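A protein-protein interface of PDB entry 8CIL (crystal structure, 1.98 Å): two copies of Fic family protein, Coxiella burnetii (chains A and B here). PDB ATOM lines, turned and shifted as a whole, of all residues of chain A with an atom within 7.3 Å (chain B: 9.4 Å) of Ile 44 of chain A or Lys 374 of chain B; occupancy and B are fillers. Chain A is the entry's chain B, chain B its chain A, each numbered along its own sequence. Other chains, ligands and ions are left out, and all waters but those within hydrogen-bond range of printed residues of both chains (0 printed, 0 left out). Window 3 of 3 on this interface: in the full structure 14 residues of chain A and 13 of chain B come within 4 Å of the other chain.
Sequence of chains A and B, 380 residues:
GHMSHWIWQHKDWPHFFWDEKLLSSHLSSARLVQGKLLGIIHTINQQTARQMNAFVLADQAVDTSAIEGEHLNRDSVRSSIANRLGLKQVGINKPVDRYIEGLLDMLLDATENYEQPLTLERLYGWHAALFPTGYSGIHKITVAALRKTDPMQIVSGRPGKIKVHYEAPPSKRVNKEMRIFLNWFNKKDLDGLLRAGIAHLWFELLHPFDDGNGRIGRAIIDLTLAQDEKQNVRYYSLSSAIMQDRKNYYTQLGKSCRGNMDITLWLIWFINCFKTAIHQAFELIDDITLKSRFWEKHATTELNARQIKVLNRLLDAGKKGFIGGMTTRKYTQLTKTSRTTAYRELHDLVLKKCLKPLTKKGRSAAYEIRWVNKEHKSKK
O of Gly 39 of chain A lies within hydrogen-bond range of OG1 of Thr 43 of chain A (2.8 Å). The backbone carbonyl oxygen (O) of Gly 39 of chain B sits at hydrogen-bond distance from the side-chain hydroxyl (OG1) of Thr 43 of chain B (2.8 Å).
Printed residues of chain B that touch a printed residue of chain A: Gly 39, Ile 40, Thr 43, Ile 44 and Lys 374. Hydrophobic or aromatic side chains of chain A within 4 Å of the printed part of chain B: Ile 40 and Ile 44.
The side-chain amino group (NZ) of Lys 374 of chain B is in hydrogen-bond range of the backbone carbonyl oxygen (O) of Thr 43 of chain A (3.1 Å). The side-chain amino group of Lys 374 of chain B lies within hydrogen-bond range of the backbone carbonyl oxygen of Ile 44 of chain A, at 3.4 Å.
Among the printed residues, pairs that only touch across the chains: Gly 39 of chain A with Gly 39 of chain B, Gly 39 of chain A with Ile 40 of chain B, Ile 40 of chain A with Gly 39 of chain B, Ile 40 of chain A with Thr 43 of chain B, Thr 43 of chain A with Ile 40 of chain B, Thr 43 of chain A with Thr 43 of chain B, Thr 43 of chain A with Ile 44 of chain B and Ile 44 of chain A with Thr 43 of chain B.
Of chain B, only Thr 43 and Lys 374 come within 4 Å of Ile 44 of chain A. Of chain A, only Thr 43 and Ile 44 come within 4 Å of Lys 374 of chain B. Thr 43 of chain A touches four residues of chain B. Of the printed residues of chain A, Ile 40 of chain B touches Gly 39 and Thr 43. Of the printed residues of chain A, Ile 44 of chain B touches Thr 43. Printed residues of chain A within 4 Å of Gly 39 of chain B: Gly 39 (3.8 Å) and Ile 40 (3.6 Å). Gln 46 of chain A touches none of the printed residues of chain B. Glu 296 of chain B touches none of the printed residues of chain A. The nearest residue of chain B that does not touch Ile 44 of chain A is Ile 44 of chain B (7.2 Å). The nearest residue of chain A that does not touch Lys 374 of chain B is Asn 45 of chain A (4.1 Å). The nearest printed residue of chain B that does not touch Gly 39 of chain A is Thr 43 of chain B (4.7 Å).
Gly 39 of chain A touches its own counterpart, Gly 39 of chain B. Gly 39 of chain A touches Ile 40 of chain B, and with the chains exchanged Ile 40 of chain A touches Gly 39 of chain B. Thr 43 of chain A touches its own counterpart, Thr 43 of chain B. Thr 43 of chain A touches Ile 44 of chain B, and with the chains exchanged Ile 44 of chain A touches Thr 43 of chain B. Of the 10 pairs that touch across the chains among the printed residues, 8 have their exchanged pair printed and touching as well.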
ATOM      1  N   LEU A  37     -10.573 -13.796 -10.137  1.00  0.00           N
ATOM      2  CA  LEU A  37     -10.114 -13.568  -8.771  1.00  0.00           C
ATOM      3  C   LEU A  37      -9.606 -12.150  -8.594  1.00  0.00           C
ATOM      4  O   LEU A  37      -9.939 -11.487  -7.620  1.00  0.00           O
ATOM      5  CB  LEU A  37      -9.001 -14.594  -8.404  1.00  0.00           C
ATOM      6  CG  LEU A  37      -8.521 -14.448  -6.948  1.00  0.00           C
ATOM      7  CD1 LEU A  37      -9.732 -14.738  -5.964  1.00  0.00           C
ATOM      8  CD2 LEU A  37      -7.351 -15.502  -6.698  1.00  0.00           C
ATOM      9  N   GLY A  39     -10.484  -9.541 -10.171  1.00  0.00           N
ATOM     10  CA  GLY A  39     -11.614  -8.624 -10.228  1.00  0.00           C
ATOM     11  C   GLY A  39     -12.391  -8.627  -8.912  1.00  0.00           C
ATOM     12  O   GLY A  39     -12.876  -7.592  -8.456  1.00  0.00           O
ATOM     13  N   ILE A  40     -12.543  -9.797  -8.320  1.00  0.00           N
ATOM     14  CA  ILE A  40     -13.156  -9.910  -6.984  1.00  0.00           C
ATOM     15  C   ILE A  40     -12.352  -9.129  -5.934  1.00  0.00           C
ATOM     16  O   ILE A  40     -12.890  -8.311  -5.183  1.00  0.00           O
ATOM     17  CB  ILE A  40     -13.297 -11.387  -6.621  1.00  0.00           C
ATOM     18  CG1 ILE A  40     -14.275 -12.053  -7.601  1.00  0.00           C
ATOM     19  CG2 ILE A  40     -13.721 -11.540  -5.156  1.00  0.00           C
ATOM     20  CD1 ILE A  40     -14.116 -13.649  -7.460  1.00  0.00           C
ATOM     21  N   ILE A  41     -11.047  -9.321  -5.911  1.00  0.00           N
ATOM     22  CA  ILE A  41     -10.205  -8.700  -4.886  1.00  0.00           C
ATOM     23  C   ILE A  41     -10.263  -7.197  -4.992  1.00  0.00           C
ATOM     24  O   ILE A  41     -10.200  -6.488  -3.982  1.00  0.00           O
ATOM     25  CB  ILE A  41      -8.728  -9.211  -4.995  1.00  0.00           C
ATOM     26  CG1 ILE A  41      -8.609 -10.703  -4.773  1.00  0.00           C
ATOM     27  CG2 ILE A  41      -7.819  -8.447  -4.027  1.00  0.00           C
ATOM     28  CD1 ILE A  41      -9.206 -11.197  -3.434  1.00  0.00           C
ATOM     29  N   HIS A  42     -10.300  -6.681  -6.235  1.00  0.00           N
ATOM     30  CA  HIS A  42     -10.397  -5.265  -6.509  1.00  0.00           C
ATOM     31  C   HIS A  42     -11.705  -4.688  -5.988  1.00  0.00           C
ATOM     32  O   HIS A  42     -11.753  -3.507  -5.641  1.00  0.00           O
ATOM     33  CB  HIS A  42     -10.236  -5.036  -8.021  1.00  0.00           C
ATOM     34  CG  HIS A  42     -10.548  -3.632  -8.495  1.00  0.00           C
ATOM     35  ND1 HIS A  42      -9.754  -2.543  -8.210  1.00  0.00           N
ATOM     36  CD2 HIS A  42     -11.558  -3.159  -9.269  1.00  0.00           C
ATOM     37  CE1 HIS A  42     -10.272  -1.457  -8.756  1.00  0.00           C
ATOM     38  NE2 HIS A  42     -11.367  -1.801  -9.410  1.00  0.00           N
ATOM     39  N   THR A  43     -12.763  -5.501  -5.890  1.00  0.00           N
ATOM     40  CA  THR A  43     -14.091  -4.941  -5.601  1.00  0.00           C
ATOM     41  C   THR A  43     -14.472  -5.057  -4.137  1.00  0.00           C
ATOM     42  O   THR A  43     -15.141  -4.172  -3.634  1.00  0.00           O
ATOM     43  CB  THR A  43     -15.136  -5.641  -6.494  1.00  0.00           C
ATOM     44  OG1 THR A  43     -14.674  -5.550  -7.853  1.00  0.00           O
ATOM     45  CG2 THR A  43     -16.511  -5.013  -6.426  1.00  0.00           C
ATOM     46  N   ILE A  44     -13.974  -6.095  -3.413  1.00  0.00           N
ATOM     47  CA  ILE A  44     -14.278  -6.258  -1.984  1.00  0.00           C
ATOM     48  C   ILE A  44     -13.635  -5.120  -1.204  1.00  0.00           C
ATOM     49  O   ILE A  44     -12.714  -4.459  -1.682  1.00  0.00           O
ATOM     50  CB  ILE A  44     -13.778  -7.624  -1.474  1.00  0.00           C
ATOM     51  CG1 ILE A  44     -12.225  -7.705  -1.607  1.00  0.00           C
ATOM     52  CG2 ILE A  44     -14.404  -8.734  -2.304  1.00  0.00           C
ATOM     53  CD1 ILE A  44     -11.547  -9.068  -1.078  1.00  0.00           C
ATOM     54  N   ASN A  45     -14.122  -4.885   0.013  1.00  0.00           N
ATOM     55  CA  ASN A  45     -13.568  -3.764   0.759  1.00  0.00           C
ATOM     56  C   ASN A  45     -12.232  -4.155   1.430  1.00  0.00           C
ATOM     57  O   ASN A  45     -11.826  -5.323   1.447  1.00  0.00           O
ATOM     58  CB  ASN A  45     -14.597  -3.219   1.775  1.00  0.00           C
ATOM     59  CG  ASN A  45     -15.022  -4.255   2.785  1.00  0.00           C
ATOM     60  OD1 ASN A  45     -14.226  -5.087   3.226  1.00  0.00           O
ATOM     61  ND2 ASN A  45     -16.251  -4.152   3.245  1.00  0.00           N
ATOM     62  N   GLN A  46     -11.517  -3.151   1.951  1.00  0.00           N
ATOM     63  CA  GLN A  46     -10.171  -3.401   2.432  1.00  0.00           C
ATOM     64  C   GLN A  46     -10.169  -4.330   3.643  1.00  0.00           C
ATOM     65  O   GLN A  46      -9.232  -5.126   3.822  1.00  0.00           O
ATOM     66  CB  GLN A  46      -9.419  -2.096   2.740  1.00  0.00           C
ATOM     67  CG  GLN A  46      -7.980  -2.408   3.239  1.00  0.00           C
ATOM     68  CD  GLN A  46      -7.052  -3.178   2.192  1.00  0.00           C
ATOM     69  OE1 GLN A  46      -7.003  -2.827   0.986  1.00  0.00           O
ATOM     70  NE2 GLN A  46      -6.327  -4.218   2.672  1.00  0.00           N
ATOM     71  N   GLN A  47     -11.218  -4.275   4.459  1.00  0.00           N
ATOM     72  CA  GLN A  47     -11.293  -5.160   5.612  1.00  0.00           C
ATOM     73  C   GLN A  47     -11.401  -6.609   5.165  1.00  0.00           C
ATOM     74  O   GLN A  47     -10.763  -7.489   5.729  1.00  0.00           O
ATOM     75  CB  GLN A  47     -12.487  -4.787   6.522  1.00  0.00           C
ATOM     76  CG  GLN A  47     -12.275  -5.036   7.993  1.00  0.00           C
ATOM     77  CD  GLN A  47     -11.530  -3.875   8.675  1.00  0.00           C
ATOM     78  OE1 GLN A  47     -10.749  -3.166   8.026  1.00  0.00           O
ATOM     79  NE2 GLN A  47     -11.783  -3.669   9.979  1.00  0.00           N
ATOM     80  N   THR A  48     -12.228  -6.879   4.165  1.00  0.00           N
ATOM     81  CA  THR A  48     -12.368  -8.242   3.679  1.00  0.00           C
ATOM     82  C   THR A  48     -11.084  -8.719   3.019  1.00  0.00           C
ATOM     83  O   THR A  48     -10.692  -9.874   3.188  1.00  0.00           O
ATOM     84  CB  THR A  48     -13.559  -8.265   2.709  1.00  0.00           C
ATOM     85  OG1 THR A  48     -14.689  -7.701   3.410  1.00  0.00           O
ATOM     86  CG2 THR A  48     -13.876  -9.674   2.204  1.00  0.00           C
ATOM     87  N   ALA A  49     -10.423  -7.843   2.236  1.00  0.00           N
ATOM     88  CA  ALA A  49      -9.144  -8.223   1.604  1.00  0.00           C
ATOM     89  C   ALA A  49      -8.059  -8.516   2.650  1.00  0.00           C
ATOM     90  O   ALA A  49      -7.245  -9.453   2.496  1.00  0.00           O
ATOM     91  CB  ALA A  49      -8.682  -7.118   0.631  1.00  0.00           C
ATOM     92  N   ARG A  50      -8.025  -7.739   3.720  1.00  0.00           N
ATOM     93  CA  ARG A  50      -7.022  -7.978   4.739  1.00  0.00           C
ATOM     94  C   ARG A  50      -7.270  -9.314   5.443  1.00  0.00           C
ATOM     95  O   ARG A  50      -6.322 -10.038   5.780  1.00  0.00           O
ATOM     96  CB  ARG A  50      -7.031  -6.838   5.774  1.00  0.00           C
ATOM     97  CG  ARG A  50      -5.937  -6.948   6.843  1.00  0.00           C
ATOM     98  CD  ARG A  50      -5.818  -5.720   7.731  1.00  0.00           C
ATOM     99  NE  ARG A  50      -5.638  -4.508   6.928  1.00  0.00           N
ATOM    100  CZ  ARG A  50      -4.467  -3.987   6.553  1.00  0.00           C
ATOM    101  NH1 ARG A  50      -3.314  -4.573   6.889  1.00  0.00           N
ATOM    102  NH2 ARG A  50      -4.454  -2.883   5.804  1.00  0.00           N
ATOM    103  N   MET A  52      -8.767 -11.912   4.024  1.00  0.00           N
ATOM    104  CA  MET A  52      -8.319 -12.881   3.032  1.00  0.00           C
ATOM    105  C   MET A  52      -6.791 -13.052   3.035  1.00  0.00           C
ATOM    106  O   MET A  52      -6.275 -14.168   2.937  1.00  0.00           O
ATOM    107  CB  MET A  52      -8.789 -12.355   1.700  1.00  0.00           C
ATOM    108  CG  MET A  52      -8.464 -13.084   0.480  1.00  0.00           C
ATOM    109  SD  MET A  52      -9.232 -14.674   0.449  1.00  0.00           S
ATOM    110  CE  MET A  52      -9.127 -14.869  -1.380  1.00  0.00           C
ATOM    111  N   TYR A 235      -3.141 -13.473  -2.930  1.00  0.00           N
ATOM    112  CA  TYR A 235      -4.512 -13.796  -2.570  1.00  0.00           C
ATOM    113  C   TYR A 235      -4.834 -15.247  -2.925  1.00  0.00           C
ATOM    114  O   TYR A 235      -5.996 -15.661  -2.885  1.00  0.00           O
ATOM    115  CB  TYR A 235      -5.477 -12.796  -3.265  1.00  0.00           C
ATOM    116  CG  TYR A 235      -5.375 -11.397  -2.625  1.00  0.00           C
ATOM    117  CD1 TYR A 235      -5.951 -11.148  -1.380  1.00  0.00           C
ATOM    118  CD2 TYR A 235      -4.699 -10.360  -3.269  1.00  0.00           C
ATOM    119  CE1 TYR A 235      -5.863  -9.870  -0.763  1.00  0.00           C
ATOM    120  CE2 TYR A 235      -4.612  -9.080  -2.712  1.00  0.00           C
ATOM    121  CZ  TYR A 235      -5.195  -8.853  -1.441  1.00  0.00           C
ATOM    122  OH  TYR A 235      -5.095  -7.621  -0.845  1.00  0.00           O
ATOM    123  N   ILE A 285     -12.856 -16.796  -0.485  1.00  0.00           N
ATOM    124  CA  ILE A 285     -13.469 -15.465  -0.494  1.00  0.00           C
ATOM    125  C   ILE A 285     -14.991 -15.580  -0.481  1.00  0.00           C
ATOM    126  O   ILE A 285     -15.692 -14.786   0.175  1.00  0.00           O
ATOM    127  CB  ILE A 285     -12.949 -14.622  -1.701  1.00  0.00           C
ATOM    128  CG1 ILE A 285     -13.466 -13.186  -1.595  1.00  0.00           C
ATOM    129  CG2 ILE A 285     -13.400 -15.209  -3.076  1.00  0.00           C
ATOM    130  CD1 ILE A 285     -13.082 -12.473  -0.295  1.00  0.00           C
ATOM    131  N   ILE A 288     -15.821 -16.289   3.178  1.00  0.00           N
ATOM    132  CA  ILE A 288     -15.675 -15.079   3.971  1.00  0.00           C
ATOM    133  C   ILE A 288     -16.878 -14.164   3.766  1.00  0.00           C
ATOM    134  O   ILE A 288     -17.531 -13.753   4.743  1.00  0.00           O
ATOM    135  CB  ILE A 288     -14.352 -14.369   3.616  1.00  0.00           C
ATOM    136  CG1 ILE A 288     -13.147 -15.210   4.026  1.00  0.00           C
ATOM    137  CG2 ILE A 288     -14.217 -13.044   4.361  1.00  0.00           C
ATOM    138  CD1 ILE A 288     -11.804 -14.607   3.501  1.00  0.00           C
ATOM    139  N   THR A 289     -17.261 -13.893   2.495  1.00  0.00           N
ATOM    140  CA  THR A 289     -18.374 -12.958   2.296  1.00  0.00           C
ATOM    141  C   THR A 289     -19.743 -13.576   2.644  1.00  0.00           C
ATOM    142  O   THR A 289     -20.646 -12.870   3.112  1.00  0.00           O
ATOM    143  CB  THR A 289     -18.363 -12.414   0.857  1.00  0.00           C
ATOM    144  OG1 THR A 289     -18.462 -13.494  -0.063  1.00  0.00           O
ATOM    145  CG2 THR A 289     -17.045 -11.654   0.575  1.00  0.00           C
ATOM    146  N   GLY B  39     -15.266 -10.776 -12.738  1.00  0.00           N
ATOM    147  CA  GLY B  39     -15.113 -10.887 -11.281  1.00  0.00           C
ATOM    148  C   GLY B  39     -15.686  -9.647 -10.594  1.00  0.00           C
ATOM    149  O   GLY B  39     -16.295  -9.734  -9.515  1.00  0.00           O
ATOM    150  N   ILE B  40     -15.456  -8.481 -11.178  1.00  0.00           N
ATOM    151  CA  ILE B  40     -16.098  -7.263 -10.648  1.00  0.00           C
ATOM    152  C   ILE B  40     -17.626  -7.425 -10.666  1.00  0.00           C
ATOM    153  O   ILE B  40     -18.321  -7.230  -9.650  1.00  0.00           O
ATOM    154  CB  ILE B  40     -15.663  -6.022 -11.456  1.00  0.00           C
ATOM    155  CG1 ILE B  40     -14.159  -5.687 -11.302  1.00  0.00           C
ATOM    156  CG2 ILE B  40     -16.584  -4.741 -11.076  1.00  0.00           C
ATOM    157  CD1 ILE B  40     -13.758  -4.597 -12.406  1.00  0.00           C
ATOM    158  N   HIS B  42     -19.502 -10.059 -10.702  1.00  0.00           N
ATOM    159  CA  HIS B  42     -19.936 -11.049  -9.728  1.00  0.00           C
ATOM    160  C   HIS B  42     -19.959 -10.472  -8.314  1.00  0.00           C
ATOM    161  O   HIS B  42     -20.697 -10.976  -7.452  1.00  0.00           O
ATOM    162  CB  HIS B  42     -18.972 -12.265  -9.826  1.00  0.00           C
ATOM    163  CG  HIS B  42     -19.229 -13.332  -8.812  1.00  0.00           C
ATOM    164  ND1 HIS B  42     -18.509 -13.444  -7.637  1.00  0.00           N
ATOM    165  CD2 HIS B  42     -20.126 -14.347  -8.798  1.00  0.00           C
ATOM    166  CE1 HIS B  42     -18.953 -14.475  -6.942  1.00  0.00           C
ATOM    167  NE2 HIS B  42     -19.919 -15.052  -7.636  1.00  0.00           N
ATOM    168  N   THR B  43     -19.123  -9.461  -8.028  1.00  0.00           N
ATOM    169  CA  THR B  43     -18.895  -8.998  -6.646  1.00  0.00           C
ATOM    170  C   THR B  43     -19.699  -7.760  -6.292  1.00  0.00           C
ATOM    171  O   THR B  43     -20.064  -7.585  -5.124  1.00  0.00           O
ATOM    172  CB  THR B  43     -17.402  -8.708  -6.376  1.00  0.00           C
ATOM    173  OG1 THR B  43     -16.615  -9.840  -6.708  1.00  0.00           O
ATOM    174  CG2 THR B  43     -17.109  -8.390  -4.903  1.00  0.00           C
ATOM    175  N   ILE B  44     -20.045  -6.908  -7.267  1.00  0.00           N
ATOM    176  CA  ILE B  44     -20.922  -5.736  -6.948  1.00  0.00           C
ATOM    177  C   ILE B  44     -22.338  -6.192  -6.604  1.00  0.00           C
ATOM    178  O   ILE B  44     -22.788  -7.263  -7.007  1.00  0.00           O
ATOM    179  CB  ILE B  44     -20.956  -4.748  -8.123  1.00  0.00           C
ATOM    180  CG1 ILE B  44     -21.564  -5.456  -9.328  1.00  0.00           C
ATOM    181  CG2 ILE B  44     -19.568  -4.274  -8.474  1.00  0.00           C
ATOM    182  CD1 ILE B  44     -21.551  -4.597 -10.640  1.00  0.00           C
ATOM    183  N   ASP B 286     -16.568   1.772 -12.989  1.00  0.00           N
ATOM    184  CA  ASP B 286     -15.928   2.629 -12.008  1.00  0.00           C
ATOM    185  C   ASP B 286     -16.793   3.870 -11.748  1.00  0.00           C
ATOM    186  O   ASP B 286     -17.056   4.224 -10.592  1.00  0.00           O
ATOM    187  CB  ASP B 286     -14.536   3.031 -12.466  1.00  0.00           C
ATOM    188  CG  ASP B 286     -13.723   3.648 -11.315  1.00  0.00           C
ATOM    189  OD1 ASP B 286     -13.548   2.983 -10.243  1.00  0.00           O
ATOM    190  OD2 ASP B 286     -13.289   4.812 -11.456  1.00  0.00           O
ATOM    191  N   THR B 289     -19.863   2.915  -9.680  1.00  0.00           N
ATOM    192  CA  THR B 289     -19.625   2.644  -8.265  1.00  0.00           C
ATOM    193  C   THR B 289     -19.208   3.907  -7.520  1.00  0.00           C
ATOM    194  O   THR B 289     -19.499   4.022  -6.332  1.00  0.00           O
ATOM    195  CB  THR B 289     -18.597   1.523  -8.086  1.00  0.00           C
ATOM    196  OG1 THR B 289     -17.371   1.898  -8.686  1.00  0.00           O
ATOM    197  CG2 THR B 289     -19.069   0.335  -8.779  1.00  0.00           C
ATOM    198  N   LEU B 290     -18.524   4.851  -8.191  1.00  0.00           N
ATOM    199  CA  LEU B 290     -18.228   6.156  -7.579  1.00  0.00           C
ATOM    200  C   LEU B 290     -19.500   6.857  -7.162  1.00  0.00           C
ATOM    201  O   LEU B 290     -19.537   7.542  -6.128  1.00  0.00           O
ATOM    202  CB  LEU B 290     -17.475   7.066  -8.554  1.00  0.00           C
ATOM    203  CG  LEU B 290     -15.990   6.734  -8.673  1.00  0.00           C
ATOM    204  CD1 LEU B 290     -15.436   7.615  -9.762  1.00  0.00           C
ATOM    205  CD2 LEU B 290     -15.259   6.929  -7.324  1.00  0.00           C
ATOM    206  N   ARG B 293     -21.164   4.988  -4.080  1.00  0.00           N
ATOM    207  CA  ARG B 293     -20.333   5.335  -2.924  1.00  0.00           C
ATOM    208  C   ARG B 293     -20.547   6.787  -2.467  1.00  0.00           C
ATOM    209  O   ARG B 293     -20.530   7.079  -1.264  1.00  0.00           O
ATOM    210  CB  ARG B 293     -18.859   5.119  -3.267  1.00  0.00           C
ATOM    211  CG  ARG B 293     -17.949   5.141  -2.055  1.00  0.00           C
ATOM    212  CD  ARG B 293     -16.494   4.708  -2.323  1.00  0.00           C
ATOM    213  NE  ARG B 293     -16.354   3.528  -3.169  1.00  0.00           N
ATOM    214  CZ  ARG B 293     -15.785   3.548  -4.369  1.00  0.00           C
ATOM    215  NH1 ARG B 293     -15.313   4.696  -4.849  1.00  0.00           N
ATOM    216  NH2 ARG B 293     -15.665   2.427  -5.079  1.00  0.00           N
ATOM    217  N   PHE B 294     -20.716   7.721  -3.412  1.00  0.00           N
ATOM    218  CA  PHE B 294     -21.032   9.092  -3.035  1.00  0.00           C
ATOM    219  C   PHE B 294     -22.342   9.129  -2.251  1.00  0.00           C
ATOM    220  O   PHE B 294     -22.459   9.839  -1.243  1.00  0.00           O
ATOM    221  CB  PHE B 294     -21.107   9.993  -4.296  1.00  0.00           C
ATOM    222  CG  PHE B 294     -21.474  11.429  -4.031  1.00  0.00           C
ATOM    223  CD1 PHE B 294     -20.494  12.415  -3.936  1.00  0.00           C
ATOM    224  CD2 PHE B 294     -22.805  11.811  -3.969  1.00  0.00           C
ATOM    225  CE1 PHE B 294     -20.814  13.773  -3.746  1.00  0.00           C
ATOM    226  CE2 PHE B 294     -23.154  13.156  -3.743  1.00  0.00           C
ATOM    227  CZ  PHE B 294     -22.156  14.140  -3.647  1.00  0.00           C
ATOM    228  N   GLU B 296     -23.845   6.757  -0.619  1.00  0.00           N
ATOM    229  CA  GLU B 296     -23.682   6.112   0.685  1.00  0.00           C
ATOM    230  C   GLU B 296     -23.129   7.083   1.718  1.00  0.00           C
ATOM    231  O   GLU B 296     -23.636   7.158   2.835  1.00  0.00           O
ATOM    232  CB  GLU B 296     -22.763   4.886   0.572  1.00  0.00           C
ATOM    233  CG  GLU B 296     -23.427   3.752  -0.128  1.00  0.00           C
ATOM    234  CD  GLU B 296     -22.466   2.638  -0.487  1.00  0.00           C
ATOM    235  OE1 GLU B 296     -21.327   2.639   0.048  1.00  0.00           O
ATOM    236  OE2 GLU B 296     -22.860   1.765  -1.299  1.00  0.00           O
ATOM    237  N   TRP B 371     -15.294  13.594  -4.920  1.00  0.00           N
ATOM    238  CA  TRP B 371     -15.483  12.121  -4.964  1.00  0.00           C
ATOM    239  C   TRP B 371     -15.120  11.449  -3.644  1.00  0.00           C
ATOM    240  O   TRP B 371     -14.220  11.936  -2.956  1.00  0.00           O
ATOM    241  CB  TRP B 371     -14.714  11.525  -6.146  1.00  0.00           C
ATOM    242  CG  TRP B 371     -15.277  11.912  -7.478  1.00  0.00           C
ATOM    243  CD1 TRP B 371     -14.698  12.719  -8.411  1.00  0.00           C
ATOM    244  CD2 TRP B 371     -16.531  11.489  -8.040  1.00  0.00           C
ATOM    245  NE1 TRP B 371     -15.508  12.839  -9.506  1.00  0.00           N
ATOM    246  CE2 TRP B 371     -16.639  12.094  -9.309  1.00  0.00           C
ATOM    247  CE3 TRP B 371     -17.571  10.666  -7.597  1.00  0.00           C
ATOM    248  CZ2 TRP B 371     -17.744  11.900 -10.135  1.00  0.00           C
ATOM    249  CZ3 TRP B 371     -18.662  10.474  -8.414  1.00  0.00           C
ATOM    250  CH2 TRP B 371     -18.745  11.085  -9.664  1.00  0.00           C
ATOM    251  N   VAL B 372     -15.825  10.374  -3.325  1.00  0.00           N
ATOM    252  CA  VAL B 372     -15.572   9.597  -2.115  1.00  0.00           C
ATOM    253  C   VAL B 372     -14.811   8.327  -2.490  1.00  0.00           C
ATOM    254  O   VAL B 372     -15.324   7.471  -3.223  1.00  0.00           O
ATOM    255  CB  VAL B 372     -16.876   9.295  -1.378  1.00  0.00           C
ATOM    256  CG1 VAL B 372     -16.625   8.452  -0.143  1.00  0.00           C
ATOM    257  CG2 VAL B 372     -17.493  10.641  -1.027  1.00  0.00           C
ATOM    258  N   ASN B 373     -13.565   8.211  -2.040  1.00  0.00           N
ATOM    259  CA  ASN B 373     -12.822   7.028  -2.432  1.00  0.00           C
ATOM    260  C   ASN B 373     -13.022   5.926  -1.388  1.00  0.00           C
ATOM    261  O   ASN B 373     -13.618   6.129  -0.326  1.00  0.00           O
ATOM    262  CB  ASN B 373     -11.353   7.394  -2.672  1.00  0.00           C
ATOM    263  CG  ASN B 373     -11.177   8.355  -3.883  1.00  0.00           C
ATOM    264  OD1 ASN B 373     -11.834   8.219  -4.925  1.00  0.00           O
ATOM    265  ND2 ASN B 373     -10.322   9.360  -3.711  1.00  0.00           N
ATOM    266  N   LYS B 374     -12.576   4.729  -1.730  1.00  0.00           N
ATOM    267  CA  LYS B 374     -12.790   3.552  -0.879  1.00  0.00           C
ATOM    268  C   LYS B 374     -12.398   3.747   0.583  1.00  0.00           C
ATOM    269  O   LYS B 374     -13.025   3.175   1.481  1.00  0.00           O
ATOM    270  CB  LYS B 374     -12.028   2.371  -1.461  1.00  0.00           C
ATOM    271  CG  LYS B 374     -12.540   1.994  -2.823  1.00  0.00           C
ATOM    272  CD  LYS B 374     -13.614   0.928  -2.713  1.00  0.00           C
ATOM    273  CE  LYS B 374     -13.016  -0.430  -2.487  1.00  0.00           C
ATOM    274  NZ  LYS B 374     -14.028  -1.508  -2.640  1.00  0.00           N
